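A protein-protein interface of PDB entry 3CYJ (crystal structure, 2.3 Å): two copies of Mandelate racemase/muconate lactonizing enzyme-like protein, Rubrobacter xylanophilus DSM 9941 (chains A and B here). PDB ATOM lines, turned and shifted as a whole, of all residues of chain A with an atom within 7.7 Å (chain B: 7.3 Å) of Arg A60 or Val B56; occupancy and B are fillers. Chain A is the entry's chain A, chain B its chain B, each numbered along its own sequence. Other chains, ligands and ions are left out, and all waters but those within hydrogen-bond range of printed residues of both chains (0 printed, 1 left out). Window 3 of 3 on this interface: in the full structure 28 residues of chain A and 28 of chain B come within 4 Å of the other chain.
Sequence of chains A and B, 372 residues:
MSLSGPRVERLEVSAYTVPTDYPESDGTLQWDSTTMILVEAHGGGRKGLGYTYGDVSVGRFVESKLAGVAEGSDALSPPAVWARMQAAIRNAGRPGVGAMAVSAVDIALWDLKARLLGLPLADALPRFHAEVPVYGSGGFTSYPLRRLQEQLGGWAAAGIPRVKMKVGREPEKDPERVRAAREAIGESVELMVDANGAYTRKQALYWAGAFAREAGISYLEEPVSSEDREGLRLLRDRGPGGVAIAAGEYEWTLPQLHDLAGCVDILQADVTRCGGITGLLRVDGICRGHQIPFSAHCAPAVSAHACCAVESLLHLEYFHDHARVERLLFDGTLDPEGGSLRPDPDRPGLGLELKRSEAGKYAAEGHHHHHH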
ATOM      1  N   VAL A  13       1.973  -3.846 -11.731  1.00  0.00           N
ATOM      2  CA  VAL A  13       1.771  -3.867 -10.308  1.00  0.00           C
ATOM      3  C   VAL A  13       0.754  -4.960  -9.970  1.00  0.00           C
ATOM      4  O   VAL A  13      -0.233  -5.105 -10.660  1.00  0.00           O
ATOM      5  CB  VAL A  13       1.202  -2.472  -9.783  1.00  0.00           C
ATOM      6  CG1 VAL A  13       1.253  -2.419  -8.281  1.00  0.00           C
ATOM      7  CG2 VAL A  13       1.968  -1.327 -10.364  1.00  0.00           C
ATOM      8  N   ILE A  37       3.040  -5.817  -2.073  1.00  0.00           N
ATOM      9  CA  ILE A  37       2.714  -5.194  -3.332  1.00  0.00           C
ATOM     10  C   ILE A  37       3.937  -5.348  -4.223  1.00  0.00           C
ATOM     11  O   ILE A  37       5.038  -5.035  -3.793  1.00  0.00           O
ATOM     12  CB  ILE A  37       2.272  -3.708  -3.174  1.00  0.00           C
ATOM     13  CG1 ILE A  37       1.058  -3.600  -2.224  1.00  0.00           C
ATOM     14  CG2 ILE A  37       1.969  -3.092  -4.537  1.00  0.00           C
ATOM     15  CD1 ILE A  37       1.438  -3.567  -0.721  1.00  0.00           C
ATOM     16  N   ASP A  55      -0.566  -1.653   2.581  1.00  0.00           N
ATOM     17  CA  ASP A  55      -1.952  -1.768   2.166  1.00  0.00           C
ATOM     18  C   ASP A  55      -2.017  -1.970   0.642  1.00  0.00           C
ATOM     19  O   ASP A  55      -1.150  -1.430  -0.096  1.00  0.00           O
ATOM     20  CB  ASP A  55      -2.774  -0.547   2.601  1.00  0.00           C
ATOM     21  CG  ASP A  55      -4.284  -0.746   2.338  1.00  0.00           C
ATOM     22  OD1 ASP A  55      -4.849  -1.722   2.890  1.00  0.00           O
ATOM     23  OD2 ASP A  55      -4.871   0.019   1.549  1.00  0.00           O
ATOM     24  N   VAL A  56      -3.038  -2.715   0.170  1.00  0.00           N
ATOM     25  CA  VAL A  56      -3.253  -2.877  -1.266  1.00  0.00           C
ATOM     26  C   VAL A  56      -3.322  -1.514  -1.933  1.00  0.00           C
ATOM     27  O   VAL A  56      -3.004  -1.392  -3.119  1.00  0.00           O
ATOM     28  CB  VAL A  56      -4.582  -3.671  -1.668  1.00  0.00           C
ATOM     29  CG1 VAL A  56      -4.455  -5.116  -1.364  1.00  0.00           C
ATOM     30  CG2 VAL A  56      -5.852  -3.104  -0.986  1.00  0.00           C
ATOM     31  N   SER A  57      -3.763  -0.486  -1.200  1.00  0.00           N
ATOM     32  CA  SER A  57      -3.855   0.836  -1.833  1.00  0.00           C
ATOM     33  C   SER A  57      -2.507   1.308  -2.376  1.00  0.00           C
ATOM     34  O   SER A  57      -2.483   2.159  -3.261  1.00  0.00           O
ATOM     35  CB  SER A  57      -4.481   1.877  -0.895  1.00  0.00           C
ATOM     36  OG  SER A  57      -3.762   1.982   0.312  1.00  0.00           O
ATOM     37  N   VAL A  58      -1.394   0.744  -1.882  1.00  0.00           N
ATOM     38  CA  VAL A  58      -0.048   1.055  -2.410  1.00  0.00           C
ATOM     39  C   VAL A  58       0.039   0.800  -3.939  1.00  0.00           C
ATOM     40  O   VAL A  58       0.569   1.635  -4.703  1.00  0.00           O
ATOM     41  CB  VAL A  58       1.060   0.247  -1.636  1.00  0.00           C
ATOM     42  CG1 VAL A  58       2.435   0.336  -2.328  1.00  0.00           C
ATOM     43  CG2 VAL A  58       1.147   0.692  -0.174  1.00  0.00           C
ATOM     44  N   GLY A  59      -0.542  -0.325  -4.393  1.00  0.00           N
ATOM     45  CA  GLY A  59      -0.604  -0.647  -5.828  1.00  0.00           C
ATOM     46  C   GLY A  59      -1.321   0.368  -6.692  1.00  0.00           C
ATOM     47  O   GLY A  59      -0.840   0.763  -7.760  1.00  0.00           O
ATOM     48  N   ARG A  60      -2.460   0.839  -6.218  1.00  0.00           N
ATOM     49  CA  ARG A  60      -3.161   1.934  -6.896  1.00  0.00           C
ATOM     50  C   ARG A  60      -2.333   3.259  -6.979  1.00  0.00           C
ATOM     51  O   ARG A  60      -2.317   3.960  -8.032  1.00  0.00           O
ATOM     52  CB  ARG A  60      -4.538   2.166  -6.205  1.00  0.00           C
ATOM     53  CG  ARG A  60      -5.436   3.108  -7.025  1.00  0.00           C
ATOM     54  CD  ARG A  60      -5.768   2.445  -8.426  1.00  0.00           C
ATOM     55  NE  ARG A  60      -6.114   3.429  -9.445  1.00  0.00           N
ATOM     56  CZ  ARG A  60      -7.351   3.893  -9.654  1.00  0.00           C
ATOM     57  NH1 ARG A  60      -8.382   3.477  -8.889  1.00  0.00           N
ATOM     58  NH2 ARG A  60      -7.557   4.781 -10.634  1.00  0.00           N
ATOM     59  N   PHE A  61      -1.630   3.599  -5.878  1.00  0.00           N
ATOM     60  CA  PHE A  61      -0.712   4.741  -5.887  1.00  0.00           C
ATOM     61  C   PHE A  61       0.377   4.611  -6.971  1.00  0.00           C
ATOM     62  O   PHE A  61       0.671   5.563  -7.682  1.00  0.00           O
ATOM     63  CB  PHE A  61      -0.040   4.924  -4.498  1.00  0.00           C
ATOM     64  CG  PHE A  61       0.604   6.291  -4.302  1.00  0.00           C
ATOM     65  CD1 PHE A  61      -0.048   7.294  -3.596  1.00  0.00           C
ATOM     66  CD2 PHE A  61       1.884   6.567  -4.832  1.00  0.00           C
ATOM     67  CE1 PHE A  61       0.564   8.589  -3.420  1.00  0.00           C
ATOM     68  CE2 PHE A  61       2.495   7.819  -4.654  1.00  0.00           C
ATOM     69  CZ  PHE A  61       1.827   8.834  -3.944  1.00  0.00           C
ATOM     70  N   VAL A  62       1.012   3.447  -7.059  1.00  0.00           N
ATOM     71  CA  VAL A  62       1.982   3.173  -8.169  1.00  0.00           C
ATOM     72  C   VAL A  62       1.357   3.400  -9.545  1.00  0.00           C
ATOM     73  O   VAL A  62       1.916   4.122 -10.397  1.00  0.00           O
ATOM     74  CB  VAL A  62       2.548   1.726  -8.111  1.00  0.00           C
ATOM     75  CG1 VAL A  62       3.436   1.405  -9.333  1.00  0.00           C
ATOM     76  CG2 VAL A  62       3.274   1.488  -6.762  1.00  0.00           C
ATOM     77  N   GLU A  63       0.177   2.804  -9.764  1.00  0.00           N
ATOM     78  CA  GLU A  63      -0.481   2.943 -11.081  1.00  0.00           C
ATOM     79  C   GLU A  63      -0.725   4.407 -11.376  1.00  0.00           C
ATOM     80  O   GLU A  63      -0.388   4.899 -12.448  1.00  0.00           O
ATOM     81  CB  GLU A  63      -1.789   2.150 -11.142  1.00  0.00           C
ATOM     82  CG  GLU A  63      -1.496   0.680 -11.097  1.00  0.00           C
ATOM     83  CD  GLU A  63      -2.704  -0.198 -10.706  1.00  0.00           C
ATOM     84  OE1 GLU A  63      -3.843   0.304 -10.477  1.00  0.00           O
ATOM     85  OE2 GLU A  63      -2.487  -1.423 -10.594  1.00  0.00           O
ATOM     86  N   SER A  64      -1.276   5.105 -10.374  1.00  0.00           N
ATOM     87  CA  SER A  64      -1.816   6.427 -10.584  1.00  0.00           C
ATOM     88  C   SER A  64      -0.719   7.456 -10.714  1.00  0.00           C
ATOM     89  O   SER A  64      -0.803   8.360 -11.557  1.00  0.00           O
ATOM     90  CB  SER A  64      -2.756   6.761  -9.439  1.00  0.00           C
ATOM     91  OG  SER A  64      -3.012   8.155  -9.407  1.00  0.00           O
ATOM     92  N   LYS A  65       0.314   7.350  -9.875  1.00  0.00           N
ATOM     93  CA  LYS A  65       1.291   8.431  -9.806  1.00  0.00           C
ATOM     94  C   LYS A  65       2.684   8.032 -10.342  1.00  0.00           C
ATOM     95  O   LYS A  65       3.406   8.876 -10.811  1.00  0.00           O
ATOM     96  CB  LYS A  65       1.456   8.949  -8.355  1.00  0.00           C
ATOM     97  CG  LYS A  65       0.249   9.647  -7.758  1.00  0.00           C
ATOM     98  CD  LYS A  65      -0.271  10.784  -8.679  1.00  0.00           C
ATOM     99  CE  LYS A  65       0.645  11.935  -8.729  1.00  0.00           C
ATOM    100  NZ  LYS A  65       0.249  12.937  -9.802  1.00  0.00           N
ATOM    101  N   LEU A  66       3.071   6.765 -10.237  1.00  0.00           N
ATOM    102  CA  LEU A  66       4.462   6.436 -10.468  1.00  0.00           C
ATOM    103  C   LEU A  66       4.772   5.845 -11.857  1.00  0.00           C
ATOM    104  O   LEU A  66       5.783   6.185 -12.460  1.00  0.00           O
ATOM    105  CB  LEU A  66       4.949   5.514  -9.327  1.00  0.00           C
ATOM    106  CG  LEU A  66       4.766   6.125  -7.903  1.00  0.00           C
ATOM    107  CD1 LEU A  66       5.417   5.273  -6.861  1.00  0.00           C
ATOM    108  CD2 LEU A  66       5.318   7.621  -7.826  1.00  0.00           C
ATOM    109  N   ALA A  67       3.889   4.983 -12.366  1.00  0.00           N
ATOM    110  CA  ALA A  67       4.139   4.273 -13.633  1.00  0.00           C
ATOM    111  C   ALA A  67       4.436   5.280 -14.728  1.00  0.00           C
ATOM    112  O   ALA A  67       5.416   5.149 -15.471  1.00  0.00           O
ATOM    113  CB  ALA A  67       2.911   3.309 -13.998  1.00  0.00           C
ATOM    114  N   ALA A  92       0.259  14.469  -3.594  1.00  0.00           N
ATOM    115  CA  ALA A  92      -0.414  13.167  -3.460  1.00  0.00           C
ATOM    116  C   ALA A  92      -0.041  12.562  -2.098  1.00  0.00           C
ATOM    117  O   ALA A  92      -0.723  11.665  -1.579  1.00  0.00           O
ATOM    118  CB  ALA A  92      -0.043  12.248  -4.609  1.00  0.00           C
ATOM    119  N   VAL A  97       2.044   5.509   2.635  1.00  0.00           N
ATOM    120  CA  VAL A  97       1.691   4.749   1.427  1.00  0.00           C
ATOM    121  C   VAL A  97       2.535   5.171   0.197  1.00  0.00           C
ATOM    122  O   VAL A  97       3.036   4.293  -0.509  1.00  0.00           O
ATOM    123  CB  VAL A  97       0.181   4.948   1.067  1.00  0.00           C
ATOM    124  CG1 VAL A  97      -0.092   4.582  -0.424  1.00  0.00           C
ATOM    125  CG2 VAL A  97      -0.680   4.182   2.027  1.00  0.00           C
ATOM    126  N   ALA A 101       5.277   3.020  -2.003  1.00  0.00           N
ATOM    127  CA  ALA A 101       5.145   2.857  -3.448  1.00  0.00           C
ATOM    128  C   ALA A 101       6.438   3.241  -4.162  1.00  0.00           C
ATOM    129  O   ALA A 101       6.946   2.465  -5.012  1.00  0.00           O
ATOM    130  CB  ALA A 101       3.957   3.670  -3.994  1.00  0.00           C
ATOM    131  N   VAL B  13     -17.444   5.269  -0.468  1.00  0.00           N
ATOM    132  CA  VAL B  13     -16.354   6.092  -0.966  1.00  0.00           C
ATOM    133  C   VAL B  13     -16.443   6.291  -2.472  1.00  0.00           C
ATOM    134  O   VAL B  13     -16.781   5.378  -3.211  1.00  0.00           O
ATOM    135  CB  VAL B  13     -14.990   5.454  -0.589  1.00  0.00           C
ATOM    136  CG1 VAL B  13     -13.843   6.402  -0.885  1.00  0.00           C
ATOM    137  CG2 VAL B  13     -15.030   5.041   0.895  1.00  0.00           C
ATOM    138  N   SER B  14     -16.143   7.494  -2.925  1.00  0.00           N
ATOM    139  CA  SER B  14     -16.059   7.774  -4.354  1.00  0.00           C
ATOM    140  C   SER B  14     -15.052   8.876  -4.584  1.00  0.00           C
ATOM    141  O   SER B  14     -14.675   9.606  -3.652  1.00  0.00           O
ATOM    142  CB  SER B  14     -17.442   8.162  -4.953  1.00  0.00           C
ATOM    143  OG  SER B  14     -17.977   9.307  -4.286  1.00  0.00           O
ATOM    144  N   ALA B  15     -14.621   9.008  -5.835  1.00  0.00           N
ATOM    145  CA  ALA B  15     -13.640  10.016  -6.194  1.00  0.00           C
ATOM    146  C   ALA B  15     -14.000  10.754  -7.495  1.00  0.00           C
ATOM    147  O   ALA B  15     -14.614  10.190  -8.393  1.00  0.00           O
ATOM    148  CB  ALA B  15     -12.206   9.401  -6.238  1.00  0.00           C
ATOM    149  N   TYR B  16     -13.579  12.005  -7.580  1.00  0.00           N
ATOM    150  CA  TYR B  16     -13.833  12.876  -8.719  1.00  0.00           C
ATOM    151  C   TYR B  16     -12.515  13.594  -9.093  1.00  0.00           C
ATOM    152  O   TYR B  16     -11.701  13.962  -8.222  1.00  0.00           O
ATOM    153  CB  TYR B  16     -14.943  13.897  -8.353  1.00  0.00           C
ATOM    154  CG  TYR B  16     -16.093  13.151  -7.715  1.00  0.00           C
ATOM    155  CD1 TYR B  16     -17.058  12.500  -8.491  1.00  0.00           C
ATOM    156  CD2 TYR B  16     -16.167  13.005  -6.316  1.00  0.00           C
ATOM    157  CE1 TYR B  16     -18.088  11.759  -7.881  1.00  0.00           C
ATOM    158  CE2 TYR B  16     -17.170  12.269  -5.710  1.00  0.00           C
ATOM    159  CZ  TYR B  16     -18.121  11.643  -6.499  1.00  0.00           C
ATOM    160  OH  TYR B  16     -19.086  10.929  -5.854  1.00  0.00           O
ATOM    161  N   THR B  17     -12.287  13.760 -10.381  1.00  0.00           N
ATOM    162  CA  THR B  17     -11.169  14.553 -10.852  1.00  0.00           C
ATOM    163  C   THR B  17     -11.721  15.709 -11.665  1.00  0.00           C
ATOM    164  O   THR B  17     -12.442  15.477 -12.613  1.00  0.00           O
ATOM    165  CB  THR B  17     -10.219  13.735 -11.728  1.00  0.00           C
ATOM    166  OG1 THR B  17      -9.770  12.579 -11.005  1.00  0.00           O
ATOM    167  CG2 THR B  17      -8.992  14.610 -12.117  1.00  0.00           C
ATOM    168  N   THR B  35      -8.138  16.212  -7.629  1.00  0.00           N
ATOM    169  CA  THR B  35      -8.901  15.044  -7.297  1.00  0.00           C
ATOM    170  C   THR B  35      -9.489  15.127  -5.864  1.00  0.00           C
ATOM    171  O   THR B  35      -8.715  15.232  -4.868  1.00  0.00           O
ATOM    172  CB  THR B  35      -8.046  13.764  -7.409  1.00  0.00           C
ATOM    173  OG1 THR B  35      -7.581  13.618  -8.747  1.00  0.00           O
ATOM    174  CG2 THR B  35      -8.901  12.539  -7.028  1.00  0.00           C
ATOM    175  N   MET B  36     -10.830  15.019  -5.772  1.00  0.00           N
ATOM    176  CA  MET B  36     -11.535  14.932  -4.464  1.00  0.00           C
ATOM    177  C   MET B  36     -11.921  13.515  -4.145  1.00  0.00           C
ATOM    178  O   MET B  36     -12.501  12.827  -4.961  1.00  0.00           O
ATOM    179  CB  MET B  36     -12.811  15.802  -4.445  1.00  0.00           C
ATOM    180  CG  MET B  36     -13.581  15.863  -3.095  1.00  0.00           C
ATOM    181  SD  MET B  36     -15.180  16.729  -3.122  1.00  0.00           S
ATOM    182  CE  MET B  36     -14.556  18.272  -2.995  1.00  0.00           C
ATOM    183  N   ILE B  37     -11.597  13.076  -2.943  1.00  0.00           N
ATOM    184  CA  ILE B  37     -12.087  11.765  -2.439  1.00  0.00           C
ATOM    185  C   ILE B  37     -13.217  11.980  -1.402  1.00  0.00           C
ATOM    186  O   ILE B  37     -13.034  12.676  -0.375  1.00  0.00           O
ATOM    187  CB  ILE B  37     -10.937  10.858  -1.889  1.00  0.00           C
ATOM    188  CG1 ILE B  37      -9.868  10.584  -2.977  1.00  0.00           C
ATOM    189  CG2 ILE B  37     -11.478   9.562  -1.444  1.00  0.00           C
ATOM    190  CD1 ILE B  37      -8.726  11.624  -2.978  1.00  0.00           C
ATOM    191  N   GLY B  54      -6.244  14.664  -2.913  1.00  0.00           N
ATOM    192  CA  GLY B  54      -4.984  13.864  -2.914  1.00  0.00           C
ATOM    193  C   GLY B  54      -5.143  12.827  -4.019  1.00  0.00           C
ATOM    194  O   GLY B  54      -5.985  12.996  -4.910  1.00  0.00           O
ATOM    195  N   ASP B  55      -4.393  11.741  -3.959  1.00  0.00           N
ATOM    196  CA  ASP B  55      -4.463  10.716  -5.004  1.00  0.00           C
ATOM    197  C   ASP B  55      -5.729   9.839  -4.870  1.00  0.00           C
ATOM    198  O   ASP B  55      -6.280   9.583  -3.753  1.00  0.00           O
ATOM    199  CB  ASP B  55      -3.201   9.831  -4.988  1.00  0.00           C
ATOM    200  CG  ASP B  55      -3.134   8.872  -6.178  1.00  0.00           C
ATOM    201  OD1 ASP B  55      -2.975   9.368  -7.310  1.00  0.00           O
ATOM    202  OD2 ASP B  55      -3.246   7.622  -6.009  1.00  0.00           O
ATOM    203  N   VAL B  56      -6.155   9.317  -6.008  1.00  0.00           N
ATOM    204  CA  VAL B  56      -7.278   8.409  -6.061  1.00  0.00           C
ATOM    205  C   VAL B  56      -7.086   7.206  -5.111  1.00  0.00           C
ATOM    206  O   VAL B  56      -8.054   6.665  -4.602  1.00  0.00           O
ATOM    207  CB  VAL B  56      -7.550   8.022  -7.570  1.00  0.00           C
ATOM    208  CG1 VAL B  56      -6.446   7.145  -8.141  1.00  0.00           C
ATOM    209  CG2 VAL B  56      -8.932   7.398  -7.748  1.00  0.00           C
ATOM    210  N   SER B  57      -5.851   6.785  -4.856  1.00  0.00           N
ATOM    211  CA  SER B  57      -5.635   5.667  -3.965  1.00  0.00           C
ATOM    212  C   SER B  57      -6.108   5.892  -2.528  1.00  0.00           C
ATOM    213  O   SER B  57      -6.250   4.948  -1.753  1.00  0.00           O
ATOM    214  CB  SER B  57      -4.144   5.311  -3.938  1.00  0.00           C
ATOM    215  OG  SER B  57      -3.343   6.472  -3.697  1.00  0.00           O
ATOM    216  N   VAL B  58      -6.376   7.145  -2.161  1.00  0.00           N
ATOM    217  CA  VAL B  58      -6.957   7.428  -0.839  1.00  0.00           C
ATOM    218  C   VAL B  58      -8.283   6.644  -0.662  1.00  0.00           C
ATOM    219  O   VAL B  58      -8.564   6.103   0.432  1.00  0.00           O
ATOM    220  CB  VAL B  58      -7.145   8.942  -0.615  1.00  0.00           C
ATOM    221  CG1 VAL B  58      -8.166   9.212   0.518  1.00  0.00           C
ATOM    222  CG2 VAL B  58      -5.821   9.645  -0.354  1.00  0.00           C
ATOM    223  N   GLY B  59      -9.081   6.549  -1.744  1.00  0.00           N
ATOM    224  CA  GLY B  59     -10.368   5.880  -1.677  1.00  0.00           C
ATOM    225  C   GLY B  59     -10.177   4.413  -1.371  1.00  0.00           C
ATOM    226  O   GLY B  59     -10.884   3.858  -0.538  1.00  0.00           O
ATOM    227  N   ARG B  60      -9.215   3.767  -2.039  1.00  0.00           N
ATOM    228  CA  ARG B  60      -8.934   2.357  -1.775  1.00  0.00           C
ATOM    229  C   ARG B  60      -8.485   2.154  -0.324  1.00  0.00           C
ATOM    230  O   ARG B  60      -8.831   1.166   0.299  1.00  0.00           O
ATOM    231  CB  ARG B  60      -7.871   1.848  -2.765  1.00  0.00           C
ATOM    232  CG  ARG B  60      -7.579   0.315  -2.647  1.00  0.00           C
ATOM    233  CD  ARG B  60      -8.700  -0.559  -3.326  1.00  0.00           C
ATOM    234  NE  ARG B  60      -9.053  -1.737  -2.542  1.00  0.00           N
ATOM    235  CZ  ARG B  60      -8.742  -2.991  -2.896  1.00  0.00           C
ATOM    236  NH1 ARG B  60      -8.080  -3.240  -4.037  1.00  0.00           N
ATOM    237  NH2 ARG B  60      -9.099  -4.014  -2.109  1.00  0.00           N
ATOM    238  N   PHE B  61      -7.701   3.093   0.210  1.00  0.00           N
ATOM    239  CA  PHE B  61      -7.237   3.056   1.593  1.00  0.00           C
ATOM    240  C   PHE B  61      -8.417   3.159   2.582  1.00  0.00           C
ATOM    241  O   PHE B  61      -8.491   2.358   3.545  1.00  0.00           O
ATOM    242  CB  PHE B  61      -6.165   4.158   1.849  1.00  0.00           C
ATOM    243  CG  PHE B  61      -5.426   4.015   3.167  1.00  0.00           C
ATOM    244  CD1 PHE B  61      -4.096   3.576   3.196  1.00  0.00           C
ATOM    245  CD2 PHE B  61      -6.043   4.355   4.373  1.00  0.00           C
ATOM    246  CE1 PHE B  61      -3.401   3.451   4.394  1.00  0.00           C
ATOM    247  CE2 PHE B  61      -5.366   4.224   5.588  1.00  0.00           C
ATOM    248  CZ  PHE B  61      -4.035   3.780   5.594  1.00  0.00           C
ATOM    249  N   VAL B  97      -1.196   9.590   2.482  1.00  0.00           N
ATOM    250  CA  VAL B  97      -2.459   8.978   2.049  1.00  0.00           C
ATOM    251  C   VAL B  97      -3.330   8.524   3.216  1.00  0.00           C
ATOM    252  O   VAL B  97      -4.532   8.843   3.252  1.00  0.00           O
ATOM    253  CB  VAL B  97      -2.222   7.771   1.060  1.00  0.00           C
ATOM    254  CG1 VAL B  97      -3.452   6.912   0.983  1.00  0.00           C
ATOM    255  CG2 VAL B  97      -1.834   8.298  -0.334  1.00  0.00           C
ATOM    256  N   ALA B 364     -13.656   9.796 -11.047  1.00  0.00           N
ATOM    257  CA  ALA B 364     -12.225   9.640 -11.354  1.00  0.00           C
ATOM    258  C   ALA B 364     -11.975   8.413 -12.253  1.00  0.00           C
ATOM    259  O   ALA B 364     -12.724   7.417 -12.144  1.00  0.00           O
ATOM    260  CB  ALA B 364     -11.449   9.517 -10.092  1.00  0.00           C
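OD2 of Asp B55 is in hydrogen-bond range of OG of Ser B57, at 2.6 Å. OG of Ser A57 is in hydrogen-bond range of OD2 of Asp A55. OE1 of Glu A63 is in salt-bridge range of NE of Arg A60 (3.999 Å).
Of the 18 printed residues of chain A, 9 touch a printed residue of chain B. Among the printed residues, 17 pairs touch across the chains. Among the printed residues, no Asp or Glu carboxylate lies within 4 Å of a Lys or Arg side-chain nitrogen of the other chain.
Val A56 touches Arg B60, and with the chains exchanged Arg A60 touches Val B56. Ser B57 touches its own counterpart, Ser A57. Ser A57 touches Phe B61, and with the chains exchanged Phe A61 touches Ser B57. Phe A61 touches Val B97, and with the chains exchanged Val A97 touches Phe B61. Positions printed for both chains: 13, 37, 55, 56, 57, 58, 59, 60, 61 and 97. Of the 17 pairs that touch across the chains among the printed residues, 12 have their exchanged pair printed and touching as well.
OD1 of Asp B55 sits at hydrogen-bond distance from OG of Ser A64 (2.4 Å).
Of the printed residues of chain B, Arg A60 touches Val B56 (3.6 Å) and Ser B57 (3.9 Å). Printed residues of chain A within 4 Å of Val B56: Arg A60 and Ser A64. No residue of chain B comes within 4 Å of Gly A59. Of the printed residues of chain A, Arg B60 touches Val A56 and Ser A57. Printed residues of chain B within 4 Å of Lys A65: Asp B55 (3.3 Å). Of the printed residues of chain A, Phe B61 touches Asp A55 (3.9 Å), Ser A57 (3.3 Å) and Val A97 (3.7 Å). Printed residues of chain B within 4 Å of Phe A61: Asp B55, Ser B57 and Val B97. The nearest residue of chain B that does not touch Arg A60 is Asp B55 (4.3 Å).
Phe B61 touches Asp A55 (CA to OD2, 3.9 Å). Ser B57 touches Ser A57. Arg A60 touches Val B56. Ser B57 touches Arg A60 (CB to CB, 3.9 Å). Val B56 touches Ser A64. Lys A65 touches Asp B55 (CG to OD1, 3.3 Å). Asp B55 touches Ala A92 (CB to CB, 3.99 Å). Val B97 touches Ala A92 (CG2 to O, 3.8 Å). Phe B61 touches Val A97 (CD1 to CG2, 3.7 Å). Val A97 touches Val B97.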
